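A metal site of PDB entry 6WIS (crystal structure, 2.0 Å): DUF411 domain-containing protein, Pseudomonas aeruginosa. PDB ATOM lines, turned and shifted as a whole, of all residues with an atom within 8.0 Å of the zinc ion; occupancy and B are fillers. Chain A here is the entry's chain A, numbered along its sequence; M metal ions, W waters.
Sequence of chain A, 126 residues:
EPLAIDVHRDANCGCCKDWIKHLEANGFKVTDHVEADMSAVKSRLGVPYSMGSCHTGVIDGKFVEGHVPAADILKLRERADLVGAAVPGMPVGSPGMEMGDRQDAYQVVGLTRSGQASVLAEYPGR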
ATOM      1  N   GLY A  14     -22.557 -30.613  11.622  1.00  0.00           N
ATOM      2  CA  GLY A  14     -22.898 -29.211  11.482  1.00  0.00           C
ATOM      3  C   GLY A  14     -21.826 -28.408  10.765  1.00  0.00           C
ATOM      4  O   GLY A  14     -22.160 -27.511   9.986  1.00  0.00           O
ATOM      5  N   CYS A  15     -20.554 -28.760  10.998  1.00  0.00           N
ATOM      6  CA  CYS A  15     -19.442 -28.028  10.379  1.00  0.00           C
ATOM      7  C   CYS A  15     -19.452 -28.143   8.855  1.00  0.00           C
ATOM      8  O   CYS A  15     -19.107 -27.177   8.163  1.00  0.00           O
ATOM      9  CB  CYS A  15     -18.107 -28.523  10.941  1.00  0.00           C
ATOM     10  SG  CYS A  15     -18.066 -30.332  10.948  1.00  0.00           S
ATOM     11  N   LYS A  17     -22.051 -28.229   6.903  1.00  0.00           N
ATOM     12  CA  LYS A  17     -23.034 -27.264   6.425  1.00  0.00           C
ATOM     13  C   LYS A  17     -22.528 -25.834   6.549  1.00  0.00           C
ATOM     14  O   LYS A  17     -22.844 -24.996   5.693  1.00  0.00           O
ATOM     15  CB  LYS A  17     -24.350 -27.423   7.217  1.00  0.00           C
ATOM     16  CG  LYS A  17     -25.107 -28.742   6.934  1.00  0.00           C
ATOM     17  CD  LYS A  17     -26.283 -28.954   7.906  1.00  0.00           C
ATOM     18  N   ASP A  18     -21.751 -25.547   7.594  1.00  0.00           N
ATOM     19  CA  ASP A  18     -21.149 -24.223   7.750  1.00  0.00           C
ATOM     20  C   ASP A  18     -20.101 -23.983   6.667  1.00  0.00           C
ATOM     21  O   ASP A  18     -20.043 -22.902   6.072  1.00  0.00           O
ATOM     22  CB  ASP A  18     -20.534 -24.111   9.156  1.00  0.00           C
ATOM     23  CG  ASP A  18     -20.058 -22.685   9.509  1.00  0.00           C
ATOM     24  OD1 ASP A  18     -20.492 -21.692   8.912  1.00  0.00           O
ATOM     25  OD2 ASP A  18     -19.241 -22.546  10.423  1.00  0.00           O
ATOM     26  N   TRP A  19     -19.259 -24.991   6.385  1.00  0.00           N
ATOM     27  CA  TRP A  19     -18.294 -24.866   5.289  1.00  0.00           C
ATOM     28  C   TRP A  19     -18.999 -24.594   3.956  1.00  0.00           C
ATOM     29  O   TRP A  19     -18.550 -23.739   3.179  1.00  0.00           O
ATOM     30  CB  TRP A  19     -17.458 -26.139   5.222  1.00  0.00           C
ATOM     31  CG  TRP A  19     -16.432 -26.192   4.185  1.00  0.00           C
ATOM     32  CD1 TRP A  19     -15.237 -25.533   4.185  1.00  0.00           C
ATOM     33  CD2 TRP A  19     -16.450 -26.988   2.992  1.00  0.00           C
ATOM     34  NE1 TRP A  19     -14.504 -25.875   3.051  1.00  0.00           N
ATOM     35  CE2 TRP A  19     -15.227 -26.786   2.315  1.00  0.00           C
ATOM     36  CE3 TRP A  19     -17.391 -27.877   2.442  1.00  0.00           C
ATOM     37  CZ2 TRP A  19     -14.919 -27.433   1.115  1.00  0.00           C
ATOM     38  CZ3 TRP A  19     -17.070 -28.531   1.232  1.00  0.00           C
ATOM     39  CH2 TRP A  19     -15.857 -28.297   0.581  1.00  0.00           C
ATOM     40  N   ILE A  20     -20.099 -25.291   3.690  1.00  0.00           N
ATOM     41  CA  ILE A  20     -20.874 -25.023   2.483  1.00  0.00           C
ATOM     42  C   ILE A  20     -21.317 -23.554   2.441  1.00  0.00           C
ATOM     43  O   ILE A  20     -21.281 -22.904   1.391  1.00  0.00           O
ATOM     44  CB  ILE A  20     -22.051 -26.000   2.395  1.00  0.00           C
ATOM     45  CG1 ILE A  20     -21.526 -27.402   2.069  1.00  0.00           C
ATOM     46  CG2 ILE A  20     -23.103 -25.511   1.394  1.00  0.00           C
ATOM     47  CD1 ILE A  20     -22.603 -28.501   2.110  1.00  0.00           C
ATOM     48  N   LYS A  21     -21.698 -22.992   3.600  1.00  0.00           N
ATOM     49  CA  LYS A  21     -22.168 -21.612   3.606  1.00  0.00           C
ATOM     50  C   LYS A  21     -21.029 -20.640   3.330  1.00  0.00           C
ATOM     51  O   LYS A  21     -21.224 -19.639   2.643  1.00  0.00           O
ATOM     52  CB  LYS A  21     -22.885 -21.294   4.918  1.00  0.00           C
ATOM     53  CG  LYS A  21     -24.293 -21.902   4.968  1.00  0.00           C
ATOM     54  CD  LYS A  21     -25.033 -21.705   6.285  1.00  0.00           C
ATOM     55  CE  LYS A  21     -25.377 -20.240   6.520  1.00  0.00           C
ATOM     56  NZ  LYS A  21     -26.307 -20.021   7.674  1.00  0.00           N
ATOM     57  N   HIS A  22     -19.812 -20.937   3.798  1.00  0.00           N
ATOM     58  CA  HIS A  22     -18.634 -20.130   3.471  1.00  0.00           C
ATOM     59  C   HIS A  22     -18.310 -20.187   1.983  1.00  0.00           C
ATOM     60  O   HIS A  22     -17.893 -19.181   1.382  1.00  0.00           O
ATOM     61  CB  HIS A  22     -17.414 -20.597   4.284  1.00  0.00           C
ATOM     62  CG  HIS A  22     -17.468 -20.233   5.737  1.00  0.00           C
ATOM     63  ND1 HIS A  22     -16.630 -19.285   6.288  1.00  0.00           N
ATOM     64  CD2 HIS A  22     -18.233 -20.699   6.746  1.00  0.00           C
ATOM     65  CE1 HIS A  22     -16.881 -19.191   7.582  1.00  0.00           C
ATOM     66  NE2 HIS A  22     -17.854 -20.018   7.885  1.00  0.00           N
ATOM     67  N   SER A  94     -10.380 -23.825  11.017  1.00  0.00           N
ATOM     68  CA  SER A  94     -10.545 -23.907   9.579  1.00  0.00           C
ATOM     69  C   SER A  94     -11.962 -23.479   9.202  1.00  0.00           C
ATOM     70  O   SER A  94     -12.856 -23.464  10.058  1.00  0.00           O
ATOM     71  CB  SER A  94     -10.237 -25.330   9.087  1.00  0.00           C
ATOM     72  OG  SER A  94     -11.171 -26.281   9.587  1.00  0.00           O
ATOM     73  N   PRO A  95     -12.191 -23.093   7.942  1.00  0.00           N
ATOM     74  CA  PRO A  95     -13.512 -22.541   7.580  1.00  0.00           C
ATOM     75  C   PRO A  95     -14.625 -23.562   7.764  1.00  0.00           C
ATOM     76  O   PRO A  95     -14.544 -24.692   7.289  1.00  0.00           O
ATOM     77  CB  PRO A  95     -13.356 -22.143   6.109  1.00  0.00           C
ATOM     78  CG  PRO A  95     -11.879 -22.147   5.822  1.00  0.00           C
ATOM     79  CD  PRO A  95     -11.223 -23.042   6.830  1.00  0.00           C
ATOM     80  N   GLY A  96     -15.683 -23.140   8.455  1.00  0.00           N
ATOM     81  CA  GLY A  96     -16.749 -24.047   8.839  1.00  0.00           C
ATOM     82  C   GLY A  96     -16.509 -24.773  10.136  1.00  0.00           C
ATOM     83  O   GLY A  96     -17.453 -25.373  10.672  1.00  0.00           O
ATOM     84  N   MET A  97     -15.304 -24.710  10.683  1.00  0.00           N
ATOM     85  CA  MET A  97     -14.925 -25.311  11.967  1.00  0.00           C
ATOM     86  C   MET A  97     -14.449 -24.205  12.923  1.00  0.00           C
ATOM     87  O   MET A  97     -13.760 -24.460  13.891  1.00  0.00           O
ATOM     88  CB  MET A  97     -13.820 -26.359  11.788  1.00  0.00           C
ATOM     89  CG  MET A  97     -14.304 -27.851  11.483  1.00  0.00           C
ATOM     90  SD  MET A  97     -15.416 -28.608  12.935  1.00  0.00           S
ATOM     91  CE  MET A  97     -13.991 -28.503  14.302  1.00  0.00           C
ATOM     92  N   GLU A  98     -14.794 -22.946  12.655  1.00  0.00           N
ATOM     93  CA  GLU A  98     -14.199 -21.884  13.458  1.00  0.00           C
ATOM     94  C   GLU A  98     -14.956 -21.735  14.776  1.00  0.00           C
ATOM     95  O   GLU A  98     -16.189 -21.775  14.814  1.00  0.00           O
ATOM     96  CB  GLU A  98     -14.153 -20.566  12.672  1.00  0.00           C
ATOM     97  CG  GLU A  98     -15.436 -19.822  12.577  1.00  0.00           C
ATOM     98  CD  GLU A  98     -16.397 -20.386  11.545  1.00  0.00           C
ATOM     99  OE1 GLU A  98     -16.129 -21.418  10.873  1.00  0.00           O
ATOM    100  OE2 GLU A  98     -17.437 -19.741  11.429  1.00  0.00           O
ATOM    101  N   MET A  99     -14.199 -21.611  15.868  1.00  0.00           N
ATOM    102  CA  MET A  99     -14.800 -21.486  17.196  1.00  0.00           C
ATOM    103  C   MET A  99     -14.001 -20.486  18.056  1.00  0.00           C
ATOM    104  O   MET A  99     -13.325 -20.887  19.008  1.00  0.00           O
ATOM    105  CB  MET A  99     -14.842 -22.853  17.891  1.00  0.00           C
ATOM    106  CG  MET A  99     -15.653 -23.900  17.140  1.00  0.00           C
ATOM    107  SD  MET A  99     -15.735 -25.624  17.961  1.00  0.00           S
ATOM    108  CE  MET A  99     -16.644 -26.496  16.514  1.00  0.00           C
HETATM  109 ZN    ZN M   1     -18.732 -20.417   9.664  1.00  0.00          ZN
HETATM  110  O   HOH W   1     -21.019 -18.836   9.576  1.00  0.00           O
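The zinc ion is bound by NE2 of His 22, OE2 of Glu 98, OD1 of Asp 18 and OD2 of Asp 18. Slightly farther from the zinc ion lies water W1 (2.8 Å).
The side-chain carboxylate (OE1) of Glu 98 lies within hydrogen-bond range of the backbone NH (N) of Gly 96 (3.0 Å).
Of the 14 residues printed, 3 come within 4 Å of the zinc ion. The nearest printed residue that does not touch the zinc ion is Gly 96 (4.2 Å).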
